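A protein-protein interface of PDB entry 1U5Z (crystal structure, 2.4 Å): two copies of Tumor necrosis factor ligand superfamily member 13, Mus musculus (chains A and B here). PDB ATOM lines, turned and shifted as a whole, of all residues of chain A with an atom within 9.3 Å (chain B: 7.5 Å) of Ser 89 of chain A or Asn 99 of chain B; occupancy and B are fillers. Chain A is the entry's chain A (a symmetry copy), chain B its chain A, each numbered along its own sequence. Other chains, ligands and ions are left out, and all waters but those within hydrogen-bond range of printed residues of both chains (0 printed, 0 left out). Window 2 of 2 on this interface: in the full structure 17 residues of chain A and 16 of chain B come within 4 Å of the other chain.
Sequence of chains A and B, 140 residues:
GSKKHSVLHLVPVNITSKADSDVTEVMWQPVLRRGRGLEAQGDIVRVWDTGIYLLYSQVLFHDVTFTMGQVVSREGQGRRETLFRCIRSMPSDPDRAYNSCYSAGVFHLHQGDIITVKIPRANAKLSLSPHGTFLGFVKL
The backbone carbonyl oxygen (O) of Gly 132 of chain B lies within hydrogen-bond range of the side-chain amide nitrogen (NE2) of Gln 58 of chain B (2.7 Å). N of Phe 61 of chain B lies within hydrogen-bond range of O of Asn 99 of chain B, 2.8 Å away. O of Met 68 of chain A lies within hydrogen-bond range of N of Arg 88 of chain A, 3.0 Å away. The side-chain sulfur (SG) of Cys 101 of chain A forms a disulfide with the side-chain sulfur (SG) of Cys 86 of chain A (2.0 Å). SG of Cys 101 of chain A sits at hydrogen-bond distance from N of Ile 87 of chain A, 3.4 Å away.
Arg 88 of chain A touches Asn 99 of chain B, but with the chains exchanged Asn 99 of chain A does not touch Arg 88 of chain B (9.0 Å). Ser 89 of chain A touches Tyr 98 of chain B, but with the chains exchanged Tyr 98 of chain A does not touch Ser 89 of chain B (13.3 Å). Ser 89 of chain A touches Asn 99 of chain B, but with the chains exchanged Asn 99 of chain A does not touch Ser 89 of chain B (9.9 Å). Of the 9 pairs that touch across the chains among the printed residues, none has its exchanged pair printed and touching as well.
Of the 18 printed residues of chain A, 5 touch a printed residue of chain B. Printed residues of chain A that touch a printed residue of chain B: Arg 85, Cys 86, Ile 87, Arg 88 and Ser 89. Of the 16 printed residues of chain B, 5 touch a printed residue of chain A. Among the printed residues, 9 pairs touch across the chains.
Of the printed residues of chain B, Arg 85 of chain A touches Gln 58 and Leu 60. Of the printed residues of chain B, Arg 88 of chain A touches Asn 99. Ser 89 of chain A touches just these residues of chain B: Tyr 98 (3.6 Å) and Asn 99 (2.7 Å). Asn 99 of chain A touches none of the printed residues of chain B. Ser 89 of chain B touches none of the printed residues of chain A. Printed residues of chain A within 4 Å of Tyr 98 of chain B: Ser 89. Printed residues of chain A within 4 Å of Asn 99 of chain B: Ile 87, Arg 88 and Ser 89. Ser 100 of chain B touches just these residues of chain A: Cys 86 (3.8 Å) and Ile 87 (3.1 Å). The nearest residue of chain B that does not touch Ser 89 of chain A is Ala 97 of chain B (4.03 Å). The nearest printed residue of chain A that does not touch Tyr 98 of chain B is Ile 87 of chain A (4.02 Å).
NE2 of Gln 58 of chain B is in hydrogen-bond range of O of Arg 85 of chain A (2.8 Å). The side-chain amide oxygen (OD1) of Asn 99 of chain B sits at hydrogen-bond distance from the side-chain hydroxyl (OG) of Ser 89 of chain A (2.7 Å). N of Ser 100 of chain B is in hydrogen-bond range of O of Ile 87 of chain A (3.1 Å).
Among the printed residues, merely in contact across the chains: Arg 85 of chain A with Leu 60 of chain B (3.2 Å), Cys 86 of chain A with Ser 100 of chain B (3.8 Å), Ile 87 of chain A with Leu 60 of chain B (3.7 Å), Ile 87 of chain A with Asn 99 of chain B (3.7 Å), Arg 88 of chain A with Asn 99 of chain B (3.97 Å) and Ser 89 of chain A with Tyr 98 of chain B (3.6 Å).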
ATOM      1  N   PHE A  61      16.147 -14.400  18.337  1.00  0.00           N
ATOM      2  CA  PHE A  61      15.296 -15.162  19.253  1.00  0.00           C
ATOM      3  C   PHE A  61      13.935 -15.499  18.637  1.00  0.00           C
ATOM      4  O   PHE A  61      13.448 -14.765  17.781  1.00  0.00           O
ATOM      5  CB  PHE A  61      15.114 -14.375  20.553  1.00  0.00           C
ATOM      6  CG  PHE A  61      16.401 -14.140  21.299  1.00  0.00           C
ATOM      7  CD1 PHE A  61      16.896 -15.100  22.162  1.00  0.00           C
ATOM      8  CD2 PHE A  61      17.125 -12.974  21.120  1.00  0.00           C
ATOM      9  CE1 PHE A  61      18.091 -14.902  22.843  1.00  0.00           C
ATOM     10  CE2 PHE A  61      18.320 -12.768  21.799  1.00  0.00           C
ATOM     11  CZ  PHE A  61      18.803 -13.735  22.665  1.00  0.00           C
ATOM     12  N   ASP A  63      11.461 -17.319  21.004  1.00  0.00           N
ATOM     13  CA  ASP A  63      10.601 -17.561  22.167  1.00  0.00           C
ATOM     14  C   ASP A  63       9.598 -16.448  22.459  1.00  0.00           C
ATOM     15  O   ASP A  63       9.839 -15.283  22.148  1.00  0.00           O
ATOM     16  CB  ASP A  63      11.453 -17.758  23.424  1.00  0.00           C
ATOM     17  CG  ASP A  63      11.883 -19.191  23.630  1.00  0.00           C
ATOM     18  OD1 ASP A  63      11.027 -20.111  23.569  1.00  0.00           O
ATOM     19  OD2 ASP A  63      13.063 -19.479  23.902  1.00  0.00           O
ATOM     20  N   VAL A  64       8.488 -16.829  23.093  1.00  0.00           N
ATOM     21  CA  VAL A  64       7.479 -15.880  23.567  1.00  0.00           C
ATOM     22  C   VAL A  64       7.705 -15.504  25.040  1.00  0.00           C
ATOM     23  O   VAL A  64       6.795 -15.012  25.706  1.00  0.00           O
ATOM     24  CB  VAL A  64       6.084 -16.470  23.376  1.00  0.00           C
ATOM     25  N   THR A  65       8.929 -15.716  25.528  1.00  0.00           N
ATOM     26  CA  THR A  65       9.296 -15.506  26.932  1.00  0.00           C
ATOM     27  C   THR A  65       9.195 -14.036  27.344  1.00  0.00           C
ATOM     28  O   THR A  65       9.242 -13.139  26.497  1.00  0.00           O
ATOM     29  CB  THR A  65      10.744 -16.005  27.148  1.00  0.00           C
ATOM     30  OG1 THR A  65      10.840 -17.390  26.788  1.00  0.00           O
ATOM     31  CG2 THR A  65      11.166 -15.985  28.615  1.00  0.00           C
ATOM     32  N   PHE A  66       9.063 -13.805  28.650  1.00  0.00           N
ATOM     33  CA  PHE A  66       8.967 -12.461  29.225  1.00  0.00           C
ATOM     34  C   PHE A  66      10.183 -11.601  28.887  1.00  0.00           C
ATOM     35  O   PHE A  66      10.046 -10.495  28.354  1.00  0.00           O
ATOM     36  CB  PHE A  66       8.793 -12.549  30.742  1.00  0.00           C
ATOM     37  N   THR A  67      11.369 -12.111  29.207  1.00  0.00           N
ATOM     38  CA  THR A  67      12.618 -11.439  28.859  1.00  0.00           C
ATOM     39  C   THR A  67      13.664 -12.432  28.352  1.00  0.00           C
ATOM     40  O   THR A  67      13.710 -13.586  28.785  1.00  0.00           O
ATOM     41  CB  THR A  67      13.157 -10.674  30.062  1.00  0.00           C
ATOM     42  N   MET A  68      14.491 -11.979  27.416  1.00  0.00           N
ATOM     43  CA  MET A  68      15.665 -12.738  27.002  1.00  0.00           C
ATOM     44  C   MET A  68      16.739 -11.895  26.318  1.00  0.00           C
ATOM     45  O   MET A  68      16.522 -10.749  25.934  1.00  0.00           O
ATOM     46  CB  MET A  68      15.277 -13.913  26.100  1.00  0.00           C
ATOM     47  CG  MET A  68      15.657 -15.265  26.681  1.00  0.00           C
ATOM     48  SD  MET A  68      15.208 -16.627  25.595  1.00  0.00           S
ATOM     49  CE  MET A  68      13.556 -16.704  25.911  1.00  0.00           C
ATOM     50  N   GLY A  69      17.906 -12.504  26.178  1.00  0.00           N
ATOM     51  CA  GLY A  69      19.034 -11.863  25.554  1.00  0.00           C
ATOM     52  C   GLY A  69      20.288 -12.703  25.655  1.00  0.00           C
ATOM     53  O   GLY A  69      20.287 -13.788  26.238  1.00  0.00           O
ATOM     54  N   ARG A  85      26.330  -7.406  27.112  1.00  0.00           N
ATOM     55  CA  ARG A  85      25.122  -8.182  26.919  1.00  0.00           C
ATOM     56  C   ARG A  85      24.089  -7.411  26.120  1.00  0.00           C
ATOM     57  O   ARG A  85      24.150  -6.188  26.002  1.00  0.00           O
ATOM     58  CB  ARG A  85      24.543  -8.593  28.264  1.00  0.00           C
ATOM     59  CG  ARG A  85      23.968  -7.461  29.046  1.00  0.00           C
ATOM     60  CD  ARG A  85      23.858  -7.752  30.525  1.00  0.00           C
ATOM     61  NE  ARG A  85      23.392  -6.567  31.229  1.00  0.00           N
ATOM     62  CZ  ARG A  85      23.251  -6.476  32.530  1.00  0.00           C
ATOM     63  NH1 ARG A  85      23.543  -7.504  33.312  1.00  0.00           N
ATOM     64  NH2 ARG A  85      22.826  -5.340  33.059  1.00  0.00           N
ATOM     65  N   CYS A  86      23.141  -8.158  25.572  1.00  0.00           N
ATOM     66  CA  CYS A  86      22.041  -7.604  24.801  1.00  0.00           C
ATOM     67  C   CYS A  86      20.740  -8.122  25.406  1.00  0.00           C
ATOM     68  O   CYS A  86      20.653  -9.289  25.739  1.00  0.00           O
ATOM     69  CB  CYS A  86      22.189  -8.049  23.348  1.00  0.00           C
ATOM     70  SG  CYS A  86      21.054  -7.258  22.220  1.00  0.00           S
ATOM     71  N   ILE A  87      19.746  -7.253  25.572  1.00  0.00           N
ATOM     72  CA  ILE A  87      18.481  -7.620  26.221  1.00  0.00           C
ATOM     73  C   ILE A  87      17.271  -7.013  25.496  1.00  0.00           C
ATOM     74  O   ILE A  87      17.334  -5.879  25.058  1.00  0.00           O
ATOM     75  CB  ILE A  87      18.479  -7.160  27.714  1.00  0.00           C
ATOM     76  CG1 ILE A  87      19.876  -7.302  28.335  1.00  0.00           C
ATOM     77  CG2 ILE A  87      17.435  -7.949  28.506  1.00  0.00           C
ATOM     78  CD1 ILE A  87      19.987  -6.825  29.766  1.00  0.00           C
ATOM     79  N   ARG A  88      16.174  -7.770  25.387  1.00  0.00           N
ATOM     80  CA  ARG A  88      14.895  -7.257  24.846  1.00  0.00           C
ATOM     81  C   ARG A  88      13.674  -7.934  25.477  1.00  0.00           C
ATOM     82  O   ARG A  88      13.662  -9.148  25.666  1.00  0.00           O
ATOM     83  CB  ARG A  88      14.849  -7.428  23.334  1.00  0.00           C
ATOM     84  N   SER A  89      12.637  -7.142  25.762  1.00  0.00           N
ATOM     85  CA  SER A  89      11.414  -7.625  26.422  1.00  0.00           C
ATOM     86  C   SER A  89      10.640  -8.642  25.580  1.00  0.00           C
ATOM     87  O   SER A  89      10.900  -8.811  24.386  1.00  0.00           O
ATOM     88  CB  SER A  89      10.490  -6.453  26.759  1.00  0.00           C
ATOM     89  OG  SER A  89      11.067  -5.615  27.742  1.00  0.00           O
ATOM     90  N   ALA A  97       7.272 -13.040  18.426  1.00  0.00           N
ATOM     91  CA  ALA A  97       8.008 -14.264  18.138  1.00  0.00           C
ATOM     92  C   ALA A  97       9.448 -13.990  17.677  1.00  0.00           C
ATOM     93  O   ALA A  97      10.400 -14.367  18.360  1.00  0.00           O
ATOM     94  CB  ALA A  97       7.265 -15.085  17.094  1.00  0.00           C
ATOM     95  N   TYR A  98       9.600 -13.329  16.528  1.00  0.00           N
ATOM     96  CA  TYR A  98      10.908 -13.161  15.881  1.00  0.00           C
ATOM     97  C   TYR A  98      11.538 -11.802  16.165  1.00  0.00           C
ATOM     98  O   TYR A  98      10.946 -10.775  15.849  1.00  0.00           O
ATOM     99  CB  TYR A  98      10.765 -13.357  14.373  1.00  0.00           C
ATOM    100  CG  TYR A  98      10.371 -14.763  14.011  1.00  0.00           C
ATOM    101  CD1 TYR A  98      11.306 -15.787  14.031  1.00  0.00           C
ATOM    102  CD2 TYR A  98       9.057 -15.081  13.674  1.00  0.00           C
ATOM    103  CE1 TYR A  98      10.939 -17.106  13.700  1.00  0.00           C
ATOM    104  CE2 TYR A  98       8.684 -16.393  13.351  1.00  0.00           C
ATOM    105  CZ  TYR A  98       9.629 -17.395  13.368  1.00  0.00           C
ATOM    106  OH  TYR A  98       9.260 -18.684  13.052  1.00  0.00           O
ATOM    107  N   ASN A  99      12.752 -11.816  16.723  1.00  0.00           N
ATOM    108  CA  ASN A  99      13.424 -10.614  17.240  1.00  0.00           C
ATOM    109  C   ASN A  99      14.917 -10.831  17.369  1.00  0.00           C
ATOM    110  O   ASN A  99      15.331 -11.747  18.058  1.00  0.00           O
ATOM    111  CB  ASN A  99      12.906 -10.257  18.641  1.00  0.00           C
ATOM    112  CG  ASN A  99      11.959  -9.098  18.634  1.00  0.00           C
ATOM    113  OD1 ASN A  99      10.834  -9.205  18.150  1.00  0.00           O
ATOM    114  ND2 ASN A  99      12.399  -7.976  19.189  1.00  0.00           N
ATOM    115  N   SER A 100      15.718  -9.989  16.726  1.00  0.00           N
ATOM    116  CA  SER A 100      17.171 -10.038  16.852  1.00  0.00           C
ATOM    117  C   SER A 100      17.681  -9.029  17.877  1.00  0.00           C
ATOM    118  O   SER A 100      17.092  -7.964  18.086  1.00  0.00           O
ATOM    119  CB  SER A 100      17.837  -9.752  15.512  1.00  0.00           C
ATOM    120  OG  SER A 100      17.629  -8.404  15.149  1.00  0.00           O
ATOM    121  N   CYS A 101      18.799  -9.379  18.487  1.00  0.00           N
ATOM    122  CA  CYS A 101      19.398  -8.589  19.549  1.00  0.00           C
ATOM    123  C   CYS A 101      20.902  -8.468  19.249  1.00  0.00           C
ATOM    124  O   CYS A 101      21.628  -9.457  19.264  1.00  0.00           O
ATOM    125  CB  CYS A 101      19.151  -9.268  20.892  1.00  0.00           C
ATOM    126  SG  CYS A 101      19.215  -8.147  22.284  1.00  0.00           S
ATOM    127  N   GLN B  58      26.007   1.700  23.530  1.00  0.00           N
ATOM    128  CA  GLN B  58      24.850   0.990  24.054  1.00  0.00           C
ATOM    129  C   GLN B  58      24.355   1.669  25.306  1.00  0.00           C
ATOM    130  O   GLN B  58      25.139   2.180  26.105  1.00  0.00           O
ATOM    131  CB  GLN B  58      25.182  -0.461  24.385  1.00  0.00           C
ATOM    132  CG  GLN B  58      23.969  -1.261  24.820  1.00  0.00           C
ATOM    133  CD  GLN B  58      24.216  -2.748  24.805  1.00  0.00           C
ATOM    134  OE1 GLN B  58      24.401  -3.328  23.741  1.00  0.00           O
ATOM    135  NE2 GLN B  58      24.191  -3.375  25.979  1.00  0.00           N
ATOM    136  N   VAL B  59      23.041   1.687  25.461  1.00  0.00           N
ATOM    137  CA  VAL B  59      22.413   2.131  26.695  1.00  0.00           C
ATOM    138  C   VAL B  59      21.385   1.075  27.083  1.00  0.00           C
ATOM    139  O   VAL B  59      20.553   0.698  26.267  1.00  0.00           O
ATOM    140  CB  VAL B  59      21.754   3.513  26.521  1.00  0.00           C
ATOM    141  CG1 VAL B  59      20.935   3.876  27.739  1.00  0.00           C
ATOM    142  CG2 VAL B  59      22.817   4.589  26.254  1.00  0.00           C
ATOM    143  N   LEU B  60      21.471   0.581  28.317  1.00  0.00           N
ATOM    144  CA  LEU B  60      20.458  -0.334  28.860  1.00  0.00           C
ATOM    145  C   LEU B  60      19.432   0.464  29.669  1.00  0.00           C
ATOM    146  O   LEU B  60      19.754   1.009  30.721  1.00  0.00           O
ATOM    147  CB  LEU B  60      21.110  -1.417  29.724  1.00  0.00           C
ATOM    148  CG  LEU B  60      20.184  -2.440  30.391  1.00  0.00           C
ATOM    149  CD1 LEU B  60      19.313  -3.185  29.402  1.00  0.00           C
ATOM    150  CD2 LEU B  60      20.999  -3.423  31.183  1.00  0.00           C
ATOM    151  N   PHE B  61      18.211   0.552  29.151  1.00  0.00           N
ATOM    152  CA  PHE B  61      17.128   1.314  29.776  1.00  0.00           C
ATOM    153  C   PHE B  61      16.326   0.471  30.772  1.00  0.00           C
ATOM    154  O   PHE B  61      16.242  -0.745  30.623  1.00  0.00           O
ATOM    155  CB  PHE B  61      16.208   1.876  28.690  1.00  0.00           C
ATOM    156  CG  PHE B  61      16.896   2.842  27.760  1.00  0.00           C
ATOM    157  CD1 PHE B  61      17.013   4.177  28.099  1.00  0.00           C
ATOM    158  CD2 PHE B  61      17.443   2.411  26.564  1.00  0.00           C
ATOM    159  CE1 PHE B  61      17.660   5.074  27.257  1.00  0.00           C
ATOM    160  CE2 PHE B  61      18.090   3.303  25.717  1.00  0.00           C
ATOM    161  CZ  PHE B  61      18.196   4.638  26.064  1.00  0.00           C
ATOM    162  N   HIS B  62      15.758   1.123  31.788  1.00  0.00           N
ATOM    163  CA  HIS B  62      14.886   0.466  32.777  1.00  0.00           C
ATOM    164  C   HIS B  62      13.460   1.026  32.818  1.00  0.00           C
ATOM    165  O   HIS B  62      12.557   0.346  33.281  1.00  0.00           O
ATOM    166  CB  HIS B  62      15.454   0.579  34.194  1.00  0.00           C
ATOM    167  CG  HIS B  62      16.867   0.109  34.330  1.00  0.00           C
ATOM    168  ND1 HIS B  62      17.234  -1.210  34.189  1.00  0.00           N
ATOM    169  CD2 HIS B  62      18.002   0.783  34.622  1.00  0.00           C
ATOM    170  CE1 HIS B  62      18.537  -1.329  34.376  1.00  0.00           C
ATOM    171  NE2 HIS B  62      19.027  -0.133  34.641  1.00  0.00           N
ATOM    172  N   ASP B  63      13.272   2.260  32.357  1.00  0.00           N
ATOM    173  CA  ASP B  63      11.985   2.958  32.447  1.00  0.00           C
ATOM    174  C   ASP B  63      10.830   2.256  31.737  1.00  0.00           C
ATOM    175  O   ASP B  63      11.033   1.537  30.761  1.00  0.00           O
ATOM    176  CB  ASP B  63      12.103   4.366  31.858  1.00  0.00           C
ATOM    177  CG  ASP B  63      12.561   5.393  32.865  1.00  0.00           C
ATOM    178  OD1 ASP B  63      11.989   5.465  33.984  1.00  0.00           O
ATOM    179  OD2 ASP B  63      13.469   6.201  32.597  1.00  0.00           O
ATOM    180  N   ARG B  88      13.763   2.841  20.866  1.00  0.00           N
ATOM    181  CA  ARG B  88      12.876   1.675  21.074  1.00  0.00           C
ATOM    182  C   ARG B  88      11.610   2.029  21.860  1.00  0.00           C
ATOM    183  O   ARG B  88      11.671   2.765  22.842  1.00  0.00           O
ATOM    184  CB  ARG B  88      13.624   0.557  21.787  1.00  0.00           C
ATOM    185  N   SER B  89      10.474   1.466  21.442  1.00  0.00           N
ATOM    186  CA  SER B  89       9.164   1.747  22.052  1.00  0.00           C
ATOM    187  C   SER B  89       9.070   1.286  23.507  1.00  0.00           C
ATOM    188  O   SER B  89       9.918   0.535  23.995  1.00  0.00           O
ATOM    189  CB  SER B  89       8.046   1.082  21.246  1.00  0.00           C
ATOM    190  OG  SER B  89       7.927   1.664  19.962  1.00  0.00           O
ATOM    191  N   ALA B  97      10.418  -3.463  31.090  1.00  0.00           N
ATOM    192  CA  ALA B  97      11.358  -2.806  31.988  1.00  0.00           C
ATOM    193  C   ALA B  97      12.780  -2.747  31.411  1.00  0.00           C
ATOM    194  O   ALA B  97      13.298  -1.660  31.149  1.00  0.00           O
ATOM    195  CB  ALA B  97      11.365  -3.509  33.339  1.00  0.00           C
ATOM    196  N   TYR B  98      13.399  -3.910  31.204  1.00  0.00           N
ATOM    197  CA  TYR B  98      14.818  -3.995  30.832  1.00  0.00           C
ATOM    198  C   TYR B  98      15.025  -4.194  29.334  1.00  0.00           C
ATOM    199  O   TYR B  98      14.539  -5.171  28.774  1.00  0.00           O
ATOM    200  CB  TYR B  98      15.485  -5.134  31.599  1.00  0.00           C
ATOM    201  CG  TYR B  98      15.525  -4.882  33.082  1.00  0.00           C
ATOM    202  CD1 TYR B  98      16.452  -4.006  33.626  1.00  0.00           C
ATOM    203  CD2 TYR B  98      14.619  -5.497  33.944  1.00  0.00           C
ATOM    204  CE1 TYR B  98      16.487  -3.763  35.013  1.00  0.00           C
ATOM    205  CE2 TYR B  98      14.644  -5.253  35.324  1.00  0.00           C
ATOM    206  CZ  TYR B  98      15.578  -4.386  35.846  1.00  0.00           C
ATOM    207  OH  TYR B  98      15.601  -4.145  37.202  1.00  0.00           O
ATOM    208  N   ASN B  99      15.780  -3.282  28.713  1.00  0.00           N
ATOM    209  CA  ASN B  99      15.926  -3.206  27.252  1.00  0.00           C
ATOM    210  C   ASN B  99      17.162  -2.423  26.863  1.00  0.00           C
ATOM    211  O   ASN B  99      17.292  -1.277  27.255  1.00  0.00           O
ATOM    212  CB  ASN B  99      14.728  -2.483  26.619  1.00  0.00           C
ATOM    213  CG  ASN B  99      13.766  -3.420  25.958  1.00  0.00           C
ATOM    214  OD1 ASN B  99      13.066  -4.180  26.624  1.00  0.00           O
ATOM    215  ND2 ASN B  99      13.706  -3.364  24.633  1.00  0.00           N
ATOM    216  N   SER B 100      18.055  -3.029  26.088  1.00  0.00           N
ATOM    217  CA  SER B 100      19.235  -2.347  25.569  1.00  0.00           C
ATOM    218  C   SER B 100      19.013  -1.840  24.147  1.00  0.00           C
ATOM    219  O   SER B 100      18.260  -2.424  23.362  1.00  0.00           O
ATOM    220  CB  SER B 100      20.440  -3.278  25.574  1.00  0.00           C
ATOM    221  OG  SER B 100      20.262  -4.302  24.618  1.00  0.00           O
ATOM    222  N   CYS B 101      19.706  -0.762  23.830  1.00  0.00           N
ATOM    223  CA  CYS B 101      19.572  -0.086  22.551  1.00  0.00           C
ATOM    224  C   CYS B 101      20.988   0.200  22.024  1.00  0.00           C
ATOM    225  O   CYS B 101      21.735   0.975  22.613  1.00  0.00           O
ATOM    226  CB  CYS B 101      18.776   1.202  22.737  1.00  0.00           C
ATOM    227  SG  CYS B 101      17.973   1.769  21.242  1.00  0.00           S
ATOM    228  N   LYS B 125      15.954   6.268  33.972  1.00  0.00           N
ATOM    229  CA  LYS B 125      16.484   5.099  34.661  1.00  0.00           C
ATOM    230  C   LYS B 125      17.307   4.262  33.693  1.00  0.00           C
ATOM    231  O   LYS B 125      16.768   3.649  32.774  1.00  0.00           O
ATOM    232  CB  LYS B 125      15.354   4.268  35.259  1.00  0.00           C
ATOM    233  CG  LYS B 125      14.630   4.986  36.370  1.00  0.00           C
ATOM    234  CD  LYS B 125      13.517   4.146  36.967  1.00  0.00           C
ATOM    235  CE  LYS B 125      12.884   4.863  38.138  1.00  0.00           C
ATOM    236  NZ  LYS B 125      11.813   4.046  38.764  1.00  0.00           N
ATOM    237  N   LEU B 126      18.618   4.262  33.899  1.00  0.00           N
ATOM    238  CA  LEU B 126      19.531   3.481  33.079  1.00  0.00           C
ATOM    239  C   LEU B 126      20.418   2.611  33.951  1.00  0.00           C
ATOM    240  O   LEU B 126      20.637   2.910  35.120  1.00  0.00           O
ATOM    241  CB  LEU B 126      20.417   4.402  32.243  1.00  0.00           C
ATOM    242  CG  LEU B 126      19.747   5.651  31.678  1.00  0.00           C
ATOM    243  CD1 LEU B 126      20.796   6.661  31.255  1.00  0.00           C
ATOM    244  CD2 LEU B 126      18.833   5.271  30.522  1.00  0.00           C
ATOM    245  N   GLY B 132      26.135  -3.452  30.265  1.00  0.00           N
ATOM    246  CA  GLY B 132      24.835  -3.024  29.771  1.00  0.00           C
ATOM    247  C   GLY B 132      24.900  -1.701  29.036  1.00  0.00           C
ATOM    248  O   GLY B 132      24.321  -1.554  27.957  1.00  0.00           O
